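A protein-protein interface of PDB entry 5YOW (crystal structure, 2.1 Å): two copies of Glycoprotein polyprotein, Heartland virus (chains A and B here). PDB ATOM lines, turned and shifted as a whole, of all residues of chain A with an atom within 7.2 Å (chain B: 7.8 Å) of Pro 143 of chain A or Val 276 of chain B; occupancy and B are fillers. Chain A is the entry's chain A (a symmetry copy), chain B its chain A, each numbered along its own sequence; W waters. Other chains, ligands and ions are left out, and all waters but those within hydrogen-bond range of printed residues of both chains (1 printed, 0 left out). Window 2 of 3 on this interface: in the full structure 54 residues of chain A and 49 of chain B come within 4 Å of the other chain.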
ATOM      1  N   ARG A  88      19.969  10.821  -7.923  1.00  0.00           N
ATOM      2  CA  ARG A  88      19.751  11.229  -6.551  1.00  0.00           C
ATOM      3  C   ARG A  88      18.634  12.266  -6.527  1.00  0.00           C
ATOM      4  O   ARG A  88      18.619  13.186  -7.350  1.00  0.00           O
ATOM      5  CB  ARG A  88      21.054  11.780  -5.932  1.00  0.00           C
ATOM      6  CG  ARG A  88      20.896  12.227  -4.470  1.00  0.00           C
ATOM      7  CD  ARG A  88      22.229  12.441  -3.736  1.00  0.00           C
ATOM      8  NE  ARG A  88      22.939  13.620  -4.232  1.00  0.00           N
ATOM      9  CZ  ARG A  88      22.808  14.855  -3.744  1.00  0.00           C
ATOM     10  NH1 ARG A  88      21.992  15.122  -2.723  1.00  0.00           N
ATOM     11  NH2 ARG A  88      23.507  15.833  -4.288  1.00  0.00           N
ATOM     12  N   ARG A  89      17.681  12.103  -5.614  1.00  0.00           N
ATOM     13  CA  ARG A  89      16.585  13.059  -5.460  1.00  0.00           C
ATOM     14  C   ARG A  89      16.559  13.525  -4.014  1.00  0.00           C
ATOM     15  O   ARG A  89      16.641  12.707  -3.090  1.00  0.00           O
ATOM     16  CB  ARG A  89      15.233  12.450  -5.904  1.00  0.00           C
ATOM     17  CG  ARG A  89      15.121  12.187  -7.442  1.00  0.00           C
ATOM     18  CD  ARG A  89      14.598  13.445  -8.220  1.00  0.00           C
ATOM     19  NE  ARG A  89      14.732  13.389  -9.692  1.00  0.00           N
ATOM     20  CZ  ARG A  89      15.853  13.601 -10.395  1.00  0.00           C
ATOM     21  NH1 ARG A  89      15.832  13.522 -11.723  1.00  0.00           N
ATOM     22  NH2 ARG A  89      16.991  13.912  -9.787  1.00  0.00           N
ATOM     23  N   CYS A  90      16.490  14.833  -3.817  1.00  0.00           N
ATOM     24  CA  CYS A  90      16.442  15.385  -2.475  1.00  0.00           C
ATOM     25  C   CYS A  90      15.210  14.879  -1.750  1.00  0.00           C
ATOM     26  O   CYS A  90      14.211  14.501  -2.367  1.00  0.00           O
ATOM     27  CB  CYS A  90      16.404  16.908  -2.508  1.00  0.00           C
ATOM     28  SG  CYS A  90      17.823  17.649  -3.272  1.00  0.00           S
ATOM     29  N   ARG A  91      15.276  14.890  -0.422  1.00  0.00           N
ATOM     30  CA  ARG A  91      14.081  14.524   0.325  1.00  0.00           C
ATOM     31  C   ARG A  91      12.991  15.554   0.050  1.00  0.00           C
ATOM     32  O   ARG A  91      13.256  16.756   0.010  1.00  0.00           O
ATOM     33  CB  ARG A  91      14.354  14.436   1.830  1.00  0.00           C
ATOM     34  CG  ARG A  91      13.037  14.162   2.563  1.00  0.00           C
ATOM     35  CD  ARG A  91      13.129  13.391   3.832  1.00  0.00           C
ATOM     36  NE  ARG A  91      13.978  12.210   3.765  1.00  0.00           N
ATOM     37  CZ  ARG A  91      14.040  11.330   4.756  1.00  0.00           C
ATOM     38  NH1 ARG A  91      13.292  11.522   5.824  1.00  0.00           N
ATOM     39  NH2 ARG A  91      14.837  10.276   4.684  1.00  0.00           N
ATOM     40  N   TRP A  92      11.769  15.064  -0.175  1.00  0.00           N
ATOM     41  CA  TRP A  92      10.555  15.781  -0.586  1.00  0.00           C
ATOM     42  C   TRP A  92      10.496  15.987  -2.097  1.00  0.00           C
ATOM     43  O   TRP A  92       9.496  16.523  -2.582  1.00  0.00           O
ATOM     44  CB  TRP A  92      10.360  17.138   0.119  1.00  0.00           C
ATOM     45  CG  TRP A  92      10.196  16.979   1.625  1.00  0.00           C
ATOM     46  CD1 TRP A  92      10.031  15.809   2.317  1.00  0.00           C
ATOM     47  CD2 TRP A  92      10.184  18.021   2.605  1.00  0.00           C
ATOM     48  NE1 TRP A  92       9.918  16.062   3.661  1.00  0.00           N
ATOM     49  CE2 TRP A  92      10.009  17.411   3.862  1.00  0.00           C
ATOM     50  CE3 TRP A  92      10.316  19.410   2.540  1.00  0.00           C
ATOM     51  CZ2 TRP A  92       9.954  18.144   5.040  1.00  0.00           C
ATOM     52  CZ3 TRP A  92      10.261  20.132   3.705  1.00  0.00           C
ATOM     53  CH2 TRP A  92      10.082  19.501   4.939  1.00  0.00           C
ATOM     54  N   CYS A  96      11.161  10.523  -3.517  1.00  0.00           N
ATOM     55  CA  CYS A  96      11.779  10.631  -2.196  1.00  0.00           C
ATOM     56  C   CYS A  96      10.952  11.479  -1.243  1.00  0.00           C
ATOM     57  O   CYS A  96      11.499  12.298  -0.486  1.00  0.00           O
ATOM     58  CB  CYS A  96      13.187  11.216  -2.307  1.00  0.00           C
ATOM     59  SG  CYS A  96      14.257  10.887  -0.839  1.00  0.00           S
ATOM     60  N   SER A  98       9.543  10.839   1.441  1.00  0.00           N
ATOM     61  CA  SER A  98       9.728  10.580   2.867  1.00  0.00           C
ATOM     62  C   SER A  98      10.892   9.616   3.095  1.00  0.00           C
ATOM     63  O   SER A  98      10.845   8.772   3.993  1.00  0.00           O
ATOM     64  CB  SER A  98       8.454  10.013   3.493  1.00  0.00           C
ATOM     65  OG  SER A  98       8.101   8.788   2.857  1.00  0.00           O
ATOM     66  N   GLY A  99      11.962   9.758   2.310  1.00  0.00           N
ATOM     67  CA  GLY A  99      13.041   8.785   2.288  1.00  0.00           C
ATOM     68  C   GLY A  99      12.833   7.786   1.162  1.00  0.00           C
ATOM     69  O   GLY A  99      11.982   7.960   0.287  1.00  0.00           O
ATOM     70  N   CYS A 100      13.648   6.740   1.161  1.00  0.00           N
ATOM     71  CA  CYS A 100      13.520   5.720   0.125  1.00  0.00           C
ATOM     72  C   CYS A 100      12.121   5.117   0.187  1.00  0.00           C
ATOM     73  O   CYS A 100      11.669   4.720   1.266  1.00  0.00           O
ATOM     74  CB  CYS A 100      14.576   4.634   0.312  1.00  0.00           C
ATOM     75  SG  CYS A 100      16.174   5.050  -0.459  1.00  0.00           S
ATOM     76  N   SER A 128      19.101   3.934  -1.809  1.00  0.00           N
ATOM     77  CA  SER A 128      20.034   4.093  -0.720  1.00  0.00           C
ATOM     78  C   SER A 128      19.903   5.522  -0.256  1.00  0.00           C
ATOM     79  O   SER A 128      19.410   6.380  -0.990  1.00  0.00           O
ATOM     80  CB  SER A 128      21.481   3.800  -1.169  1.00  0.00           C
ATOM     81  OG  SER A 128      21.569   2.505  -1.773  1.00  0.00           O
ATOM     82  N   ASP A 129      20.302   5.760   0.981  1.00  0.00           N
ATOM     83  CA  ASP A 129      20.337   7.115   1.498  1.00  0.00           C
ATOM     84  C   ASP A 129      21.549   7.841   0.935  1.00  0.00           C
ATOM     85  O   ASP A 129      22.616   7.254   0.771  1.00  0.00           O
ATOM     86  CB  ASP A 129      20.356   7.074   3.026  1.00  0.00           C
ATOM     87  CG  ASP A 129      19.053   6.558   3.605  1.00  0.00           C
ATOM     88  OD1 ASP A 129      17.995   6.769   2.981  1.00  0.00           O
ATOM     89  OD2 ASP A 129      19.064   5.937   4.681  1.00  0.00           O
ATOM     90  N   GLY A 130      21.355   9.109   0.567  1.00  0.00           N
ATOM     91  CA  GLY A 130      22.434   9.983   0.167  1.00  0.00           C
ATOM     92  C   GLY A 130      22.459  11.187   1.100  1.00  0.00           C
ATOM     93  O   GLY A 130      21.541  11.397   1.897  1.00  0.00           O
ATOM     94  N   CYS A 131      23.516  11.979   0.999  1.00  0.00           N
ATOM     95  CA  CYS A 131      23.618  13.132   1.887  1.00  0.00           C
ATOM     96  C   CYS A 131      22.630  14.211   1.473  1.00  0.00           C
ATOM     97  O   CYS A 131      22.322  14.380   0.296  1.00  0.00           O
ATOM     98  CB  CYS A 131      25.034  13.692   1.905  1.00  0.00           C
ATOM     99  SG  CYS A 131      25.683  14.121   0.322  1.00  0.00           S
ATOM    100  N   GLY A 132      22.101  14.921   2.463  1.00  0.00           N
ATOM    101  CA  GLY A 132      21.172  16.001   2.241  1.00  0.00           C
ATOM    102  C   GLY A 132      21.803  17.353   2.504  1.00  0.00           C
ATOM    103  O   GLY A 132      23.021  17.491   2.622  1.00  0.00           O
ATOM    104  N   GLY A 133      20.945  18.369   2.568  1.00  0.00           N
ATOM    105  CA  GLY A 133      21.397  19.694   2.934  1.00  0.00           C
ATOM    106  C   GLY A 133      22.099  20.438   1.810  1.00  0.00           C
ATOM    107  O   GLY A 133      22.412  19.904   0.741  1.00  0.00           O
ATOM    108  N   CYS A 138      20.824  20.241  -1.632  1.00  0.00           N
ATOM    109  CA  CYS A 138      19.433  20.001  -1.289  1.00  0.00           C
ATOM    110  C   CYS A 138      18.988  21.017  -0.256  1.00  0.00           C
ATOM    111  O   CYS A 138      19.744  21.347   0.654  1.00  0.00           O
ATOM    112  CB  CYS A 138      19.236  18.589  -0.744  1.00  0.00           C
ATOM    113  SG  CYS A 138      19.395  17.291  -1.993  1.00  0.00           S
ATOM    114  N   ASN A 140      16.275  20.499   1.846  1.00  0.00           N
ATOM    115  CA  ASN A 140      15.983  19.701   3.028  1.00  0.00           C
ATOM    116  C   ASN A 140      17.256  19.016   3.530  1.00  0.00           C
ATOM    117  O   ASN A 140      17.976  18.370   2.760  1.00  0.00           O
ATOM    118  CB  ASN A 140      14.919  18.656   2.688  1.00  0.00           C
ATOM    119  CG  ASN A 140      14.398  17.905   3.907  1.00  0.00           C
ATOM    120  OD1 ASN A 140      15.148  17.518   4.794  1.00  0.00           O
ATOM    121  ND2 ASN A 140      13.092  17.676   3.934  1.00  0.00           N
ATOM    122  N   ALA A 141      17.502  19.107   4.837  1.00  0.00           N
ATOM    123  CA  ALA A 141      18.750  18.611   5.394  1.00  0.00           C
ATOM    124  C   ALA A 141      18.720  17.116   5.652  1.00  0.00           C
ATOM    125  O   ALA A 141      19.780  16.527   5.867  1.00  0.00           O
ATOM    126  CB  ALA A 141      19.081  19.347   6.689  1.00  0.00           C
ATOM    127  N   ALA A 142      17.536  16.495   5.651  1.00  0.00           N
ATOM    128  CA  ALA A 142      17.442  15.048   5.831  1.00  0.00           C
ATOM    129  C   ALA A 142      18.079  14.321   4.647  1.00  0.00           C
ATOM    130  O   ALA A 142      18.341  14.923   3.598  1.00  0.00           O
ATOM    131  CB  ALA A 142      15.976  14.632   6.013  1.00  0.00           C
ATOM    132  N   PRO A 143      18.371  13.029   4.802  1.00  0.00           N
ATOM    133  CA  PRO A 143      19.047  12.293   3.722  1.00  0.00           C
ATOM    134  C   PRO A 143      18.248  12.293   2.419  1.00  0.00           C
ATOM    135  O   PRO A 143      17.018  12.217   2.421  1.00  0.00           O
ATOM    136  CB  PRO A 143      19.181  10.879   4.294  1.00  0.00           C
ATOM    137  CG  PRO A 143      19.195  11.093   5.796  1.00  0.00           C
ATOM    138  CD  PRO A 143      18.264  12.226   6.035  1.00  0.00           C
ATOM    139  N   SER A 144      18.966  12.410   1.303  1.00  0.00           N
ATOM    140  CA  SER A 144      18.375  12.289  -0.021  1.00  0.00           C
ATOM    141  C   SER A 144      18.214  10.810  -0.373  1.00  0.00           C
ATOM    142  O   SER A 144      18.591   9.920   0.396  1.00  0.00           O
ATOM    143  CB  SER A 144      19.238  13.010  -1.048  1.00  0.00           C
ATOM    144  OG  SER A 144      20.600  12.613  -0.906  1.00  0.00           O
ATOM    145  N   CYS A 145      17.644  10.537  -1.545  1.00  0.00           N
ATOM    146  CA  CYS A 145      17.467   9.181  -2.048  1.00  0.00           C
ATOM    147  C   CYS A 145      18.367   8.967  -3.258  1.00  0.00           C
ATOM    148  O   CYS A 145      18.399   9.806  -4.156  1.00  0.00           O
ATOM    149  CB  CYS A 145      16.010   8.943  -2.459  1.00  0.00           C
ATOM    150  SG  CYS A 145      14.791   8.956  -1.125  1.00  0.00           S
ATOM    151  N   SER B  86      19.738  -4.255  11.984  1.00  0.00           N
ATOM    152  CA  SER B  86      20.612  -3.149  12.339  1.00  0.00           C
ATOM    153  C   SER B  86      19.923  -2.319  13.398  1.00  0.00           C
ATOM    154  O   SER B  86      18.697  -2.351  13.529  1.00  0.00           O
ATOM    155  CB  SER B  86      20.991  -2.276  11.136  1.00  0.00           C
ATOM    156  OG  SER B  86      19.859  -1.643  10.581  1.00  0.00           O
ATOM    157  N   VAL B  87      20.734  -1.613  14.180  1.00  0.00           N
ATOM    158  CA  VAL B  87      20.270  -0.571  15.099  1.00  0.00           C
ATOM    159  C   VAL B  87      21.304   0.538  15.057  1.00  0.00           C
ATOM    160  O   VAL B  87      22.504   0.274  14.932  1.00  0.00           O
ATOM    161  CB  VAL B  87      20.077  -1.090  16.544  1.00  0.00           C
ATOM    162  CG1 VAL B  87      21.412  -1.488  17.160  1.00  0.00           C
ATOM    163  CG2 VAL B  87      19.415  -0.043  17.413  1.00  0.00           C
ATOM    164  N   ARG B  88      20.837   1.780  15.125  1.00  0.00           N
ATOM    165  CA  ARG B  88      21.682   2.954  15.054  1.00  0.00           C
ATOM    166  C   ARG B  88      21.650   3.655  16.407  1.00  0.00           C
ATOM    167  O   ARG B  88      20.578   3.822  16.998  1.00  0.00           O
ATOM    168  CB  ARG B  88      21.219   3.891  13.915  1.00  0.00           C
ATOM    169  CG  ARG B  88      22.078   5.157  13.778  1.00  0.00           C
ATOM    170  CD  ARG B  88      21.866   5.915  12.458  1.00  0.00           C
ATOM    171  NE  ARG B  88      20.552   6.555  12.405  1.00  0.00           N
ATOM    172  CZ  ARG B  88      20.286   7.795  12.819  1.00  0.00           C
ATOM    173  NH1 ARG B  88      21.235   8.581  13.331  1.00  0.00           N
ATOM    174  NH2 ARG B  88      19.052   8.251  12.717  1.00  0.00           N
ATOM    175  N   ARG B  89      22.819   4.033  16.916  1.00  0.00           N
ATOM    176  CA  ARG B  89      22.913   4.757  18.183  1.00  0.00           C
ATOM    177  C   ARG B  89      23.689   6.040  17.941  1.00  0.00           C
ATOM    178  O   ARG B  89      24.745   6.022  17.296  1.00  0.00           O
ATOM    179  CB  ARG B  89      23.552   3.886  19.291  1.00  0.00           C
ATOM    180  CG  ARG B  89      22.663   2.684  19.756  1.00  0.00           C
ATOM    181  CD  ARG B  89      21.675   3.091  20.904  1.00  0.00           C
ATOM    182  NE  ARG B  89      20.608   2.112  21.207  1.00  0.00           N
ATOM    183  CZ  ARG B  89      19.483   1.922  20.503  1.00  0.00           C
ATOM    184  NH1 ARG B  89      18.601   1.004  20.891  1.00  0.00           N
ATOM    185  NH2 ARG B  89      19.219   2.654  19.428  1.00  0.00           N
ATOM    186  N   GLY B 130      27.101   6.077  10.741  1.00  0.00           N
ATOM    187  CA  GLY B 130      25.850   6.582  10.222  1.00  0.00           C
ATOM    188  C   GLY B 130      25.842   8.100  10.354  1.00  0.00           C
ATOM    189  O   GLY B 130      26.712   8.689  11.002  1.00  0.00           O
ATOM    190  N   CYS B 131      24.857   8.733   9.737  1.00  0.00           N
ATOM    191  CA  CYS B 131      24.809  10.189   9.796  1.00  0.00           C
ATOM    192  C   CYS B 131      24.388  10.652  11.182  1.00  0.00           C
ATOM    193  O   CYS B 131      23.610   9.993  11.867  1.00  0.00           O
ATOM    194  CB  CYS B 131      23.868  10.755   8.741  1.00  0.00           C
ATOM    195  SG  CYS B 131      22.223  10.121   8.797  1.00  0.00           S
ATOM    196  N   GLY B 132      24.943  11.781  11.609  1.00  0.00           N
ATOM    197  CA  GLY B 132      24.628  12.372  12.885  1.00  0.00           C
ATOM    198  C   GLY B 132      23.791  13.626  12.736  1.00  0.00           C
ATOM    199  O   GLY B 132      23.239  13.919  11.675  1.00  0.00           O
ATOM    200  N   ALA B 134      20.872  16.717  13.984  1.00  0.00           N
ATOM    201  CA  ALA B 134      19.417  16.810  14.034  1.00  0.00           C
ATOM    202  C   ALA B 134      18.778  16.223  12.783  1.00  0.00           C
ATOM    203  O   ALA B 134      17.707  15.612  12.855  1.00  0.00           O
ATOM    204  CB  ALA B 134      18.999  18.277  14.202  1.00  0.00           C
ATOM    205  N   ALA B 135      19.410  16.425  11.626  1.00  0.00           N
ATOM    206  CA  ALA B 135      18.869  15.905  10.374  1.00  0.00           C
ATOM    207  C   ALA B 135      18.660  14.399  10.432  1.00  0.00           C
ATOM    208  O   ALA B 135      17.755  13.878   9.773  1.00  0.00           O
ATOM    209  CB  ALA B 135      19.801  16.248   9.212  1.00  0.00           C
ATOM    210  N   CYS B 136      19.478  13.688  11.212  1.00  0.00           N
ATOM    211  CA  CYS B 136      19.343  12.247  11.397  1.00  0.00           C
ATOM    212  C   CYS B 136      18.941  11.893  12.830  1.00  0.00           C
ATOM    213  O   CYS B 136      19.257  10.808  13.324  1.00  0.00           O
ATOM    214  CB  CYS B 136      20.641  11.547  11.001  1.00  0.00           C
ATOM    215  SG  CYS B 136      21.064  11.758   9.239  1.00  0.00           S
ATOM    216  N   GLY B 137      18.250  12.801  13.516  1.00  0.00           N
ATOM    217  CA  GLY B 137      17.661  12.468  14.800  1.00  0.00           C
ATOM    218  C   GLY B 137      18.615  12.406  15.967  1.00  0.00           C
ATOM    219  O   GLY B 137      18.307  11.754  16.972  1.00  0.00           O
ATOM    220  N   SER B 144      26.928   8.840  13.820  1.00  0.00           N
ATOM    221  CA  SER B 144      26.334   7.841  14.695  1.00  0.00           C
ATOM    222  C   SER B 144      26.962   6.477  14.410  1.00  0.00           C
ATOM    223  O   SER B 144      27.812   6.331  13.525  1.00  0.00           O
ATOM    224  CB  SER B 144      24.824   7.806  14.500  1.00  0.00           C
ATOM    225  OG  SER B 144      24.513   7.720  13.112  1.00  0.00           O
ATOM    226  N   CYS B 145      26.548   5.462  15.166  1.00  0.00           N
ATOM    227  CA  CYS B 145      27.009   4.093  14.984  1.00  0.00           C
ATOM    228  C   CYS B 145      25.860   3.232  14.474  1.00  0.00           C
ATOM    229  O   CYS B 145      24.759   3.293  15.017  1.00  0.00           O
ATOM    230  CB  CYS B 145      27.519   3.514  16.308  1.00  0.00           C
ATOM    231  SG  CYS B 145      29.011   4.272  16.990  1.00  0.00           S
ATOM    232  N   ILE B 146      26.114   2.412  13.465  1.00  0.00           N
ATOM    233  CA  ILE B 146      25.139   1.426  13.015  1.00  0.00           C
ATOM    234  C   ILE B 146      25.693   0.048  13.326  1.00  0.00           C
ATOM    235  O   ILE B 146      26.665  -0.399  12.708  1.00  0.00           O
ATOM    236  CB  ILE B 146      24.806   1.567  11.524  1.00  0.00           C
ATOM    237  CG1 ILE B 146      24.222   2.975  11.273  1.00  0.00           C
ATOM    238  CG2 ILE B 146      23.782   0.496  11.142  1.00  0.00           C
ATOM    239  CD1 ILE B 146      23.936   3.313   9.816  1.00  0.00           C
ATOM    240  N   GLU B 273      22.395  -3.808   3.047  1.00  0.00           N
ATOM    241  CA  GLU B 273      22.533  -2.413   2.658  1.00  0.00           C
ATOM    242  C   GLU B 273      22.079  -1.578   3.837  1.00  0.00           C
ATOM    243  O   GLU B 273      20.926  -1.685   4.256  1.00  0.00           O
ATOM    244  CB  GLU B 273      21.700  -2.087   1.414  1.00  0.00           C
ATOM    245  CG  GLU B 273      21.823  -0.638   0.942  1.00  0.00           C
ATOM    246  CD  GLU B 273      20.624  -0.146   0.128  1.00  0.00           C
ATOM    247  OE1 GLU B 273      20.013  -0.921  -0.640  1.00  0.00           O
ATOM    248  OE2 GLU B 273      20.305   1.051   0.252  1.00  0.00           O
ATOM    249  N   LEU B 274      22.984  -0.770   4.386  1.00  0.00           N
ATOM    250  CA  LEU B 274      22.645   0.062   5.533  1.00  0.00           C
ATOM    251  C   LEU B 274      22.010   1.339   5.026  1.00  0.00           C
ATOM    252  O   LEU B 274      22.550   1.998   4.127  1.00  0.00           O
ATOM    253  CB  LEU B 274      23.877   0.390   6.382  1.00  0.00           C
ATOM    254  CG  LEU B 274      24.627  -0.806   6.998  1.00  0.00           C
ATOM    255  CD1 LEU B 274      25.706  -0.319   7.973  1.00  0.00           C
ATOM    256  CD2 LEU B 274      23.667  -1.727   7.714  1.00  0.00           C
ATOM    257  N   ARG B 275      20.857   1.672   5.576  1.00  0.00           N
ATOM    258  CA  ARG B 275      20.277   2.973   5.351  1.00  0.00           C
ATOM    259  C   ARG B 275      20.248   3.673   6.692  1.00  0.00           C
ATOM    260  O   ARG B 275      20.687   3.114   7.707  1.00  0.00           O
ATOM    261  CB  ARG B 275      18.905   2.851   4.680  1.00  0.00           C
ATOM    262  CG  ARG B 275      19.049   2.085   3.375  1.00  0.00           C
ATOM    263  CD  ARG B 275      17.926   2.321   2.393  1.00  0.00           C
ATOM    264  NE  ARG B 275      16.674   1.741   2.849  1.00  0.00           N
ATOM    265  CZ  ARG B 275      15.744   1.222   2.051  1.00  0.00           C
ATOM    266  NH1 ARG B 275      15.916   1.157   0.730  1.00  0.00           N
ATOM    267  NH2 ARG B 275      14.644   0.742   2.590  1.00  0.00           N
ATOM    268  N   VAL B 276      19.759   4.911   6.693  1.00  0.00           N
ATOM    269  CA  VAL B 276      19.876   5.714   7.899  1.00  0.00           C
ATOM    270  C   VAL B 276      19.132   5.038   9.041  1.00  0.00           C
ATOM    271  O   VAL B 276      19.692   4.825  10.124  1.00  0.00           O
ATOM    272  CB  VAL B 276      19.391   7.152   7.640  1.00  0.00           C
ATOM    273  CG1 VAL B 276      19.147   7.874   8.936  1.00  0.00           C
ATOM    274  CG2 VAL B 276      20.455   7.891   6.813  1.00  0.00           C
ATOM    275  N   ASP B 277      17.900   4.591   8.783  1.00  0.00           N
ATOM    276  CA  ASP B 277      17.073   4.024   9.841  1.00  0.00           C
ATOM    277  C   ASP B 277      16.565   2.611   9.546  1.00  0.00           C
ATOM    278  O   ASP B 277      15.566   2.198  10.135  1.00  0.00           O
ATOM    279  CB  ASP B 277      15.911   4.963  10.122  1.00  0.00           C
ATOM    280  CG  ASP B 277      16.389   6.318  10.589  1.00  0.00           C
ATOM    281  OD1 ASP B 277      17.225   6.350  11.523  1.00  0.00           O
ATOM    282  OD2 ASP B 277      15.974   7.334  10.002  1.00  0.00           O
ATOM    283  N   ASP B 278      17.230   1.857   8.678  1.00  0.00           N
ATOM    284  CA  ASP B 278      16.889   0.448   8.459  1.00  0.00           C
ATOM    285  C   ASP B 278      17.995  -0.189   7.637  1.00  0.00           C
ATOM    286  O   ASP B 278      19.008   0.442   7.305  1.00  0.00           O
ATOM    287  CB  ASP B 278      15.517   0.245   7.782  1.00  0.00           C
ATOM    288  CG  ASP B 278      15.475   0.711   6.316  1.00  0.00           C
ATOM    289  OD1 ASP B 278      16.415   1.378   5.849  1.00  0.00           O
ATOM    290  OD2 ASP B 278      14.480   0.402   5.620  1.00  0.00           O
ATOM    291  N   ALA B 279      17.802  -1.464   7.324  1.00  0.00           N
ATOM    292  CA  ALA B 279      18.748  -2.134   6.469  1.00  0.00           C
ATOM    293  C   ALA B 279      17.962  -2.987   5.482  1.00  0.00           C
ATOM    294  O   ALA B 279      16.832  -3.409   5.744  1.00  0.00           O
ATOM    295  CB  ALA B 279      19.750  -2.946   7.286  1.00  0.00           C
HETATM  296  O   HOH W   1      22.076   3.799   2.310  1.00  0.00           O
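Among the printed residues, pairs that only touch across the chains: Cys 100 of chain A with Arg 275 of chain B, Asp 129 of chain A with Arg 275 of chain B, Ala 141 of chain A with Ala 135 of chain B, Pro 143 of chain A with Cys 136 of chain B and Pro 143 of chain A with Val 276 of chain B.
OD2 of Asp 129 of chain A sits close to N of Val 276 of chain B (2.4 Å). OE2 of Glu 273 of chain B lies within hydrogen-bond range of OG of Ser 128 of chain A (2.8 Å).
Positions printed for both chains: 88, 89, 130, 131, 132, 144 and 145. Of the 7 pairs that touch across the chains among the printed residues, none has its exchanged pair printed and touching as well.
Of the 21 printed residues of chain B, 5 touch a printed residue of chain A. Printed residues of chain B that touch a printed residue of chain A: Ala 135, Cys 136, Glu 273, Arg 275 and Val 276. Hydrophobic or aromatic side chains of chain B that line the printed part of chain A: Ala 135 and Val 276. Among the printed residues, 7 pairs touch across the chains. Among the printed residues, no Asp or Glu carboxylate lies within 4 Å of a Lys or Arg side-chain nitrogen of the other chain.
Water W1 bridges the backbone carbonyl oxygen (O) of Leu 274 of chain B (2.6 Å) and the backbone NH (N) of Asp 129 of chain A (3.0 Å).
Of the printed residues of chain B, Ser 128 of chain A touches Glu 273. Printed residues of chain B within 4 Å of Asp 129 of chain A: Arg 275 (3.1 Å) and Val 276 (2.4 Å). Printed residues of chain B within 4 Å of Ala 141 of chain A: Ala 135. No residue of chain B comes within 4 Å of Ala 142 of chain A. Of chain B, only Cys 136 (3.97 Å) and Val 276 (3.6 Å) come within 4 Å of Pro 143 of chain A. Of the printed residues of chain A, Val 276 of chain B touches Asp 129 (2.4 Å) and Pro 143 (3.6 Å).
The guanidinium group of Arg 275 of chain B is in salt-bridge range of the side-chain carboxylate of Asp 278 of chain B, 3.0 Å away. The backbone carbonyl oxygen (O) of Cys 136 of chain B sits at hydrogen-bond distance from the guanidinium group (NH2) of Arg 88 of chain B (2.6 Å). N of Cys 100 of chain A is in hydrogen-bond range of SG of Cys 145 of chain A. The side-chain sulfur of Cys 96 of chain A is disulfide-bonded to the side-chain sulfur of Cys 145 of chain A, at 2.0 Å. SG of Cys 131 of chain B forms a disulfide with SG of Cys 136 of chain B, at 2.1 Å. The guanidinium group of Arg 91 of chain A sits at hydrogen-bond distance from the backbone carbonyl oxygen of Pro 143 of chain A, 3.3 Å away.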
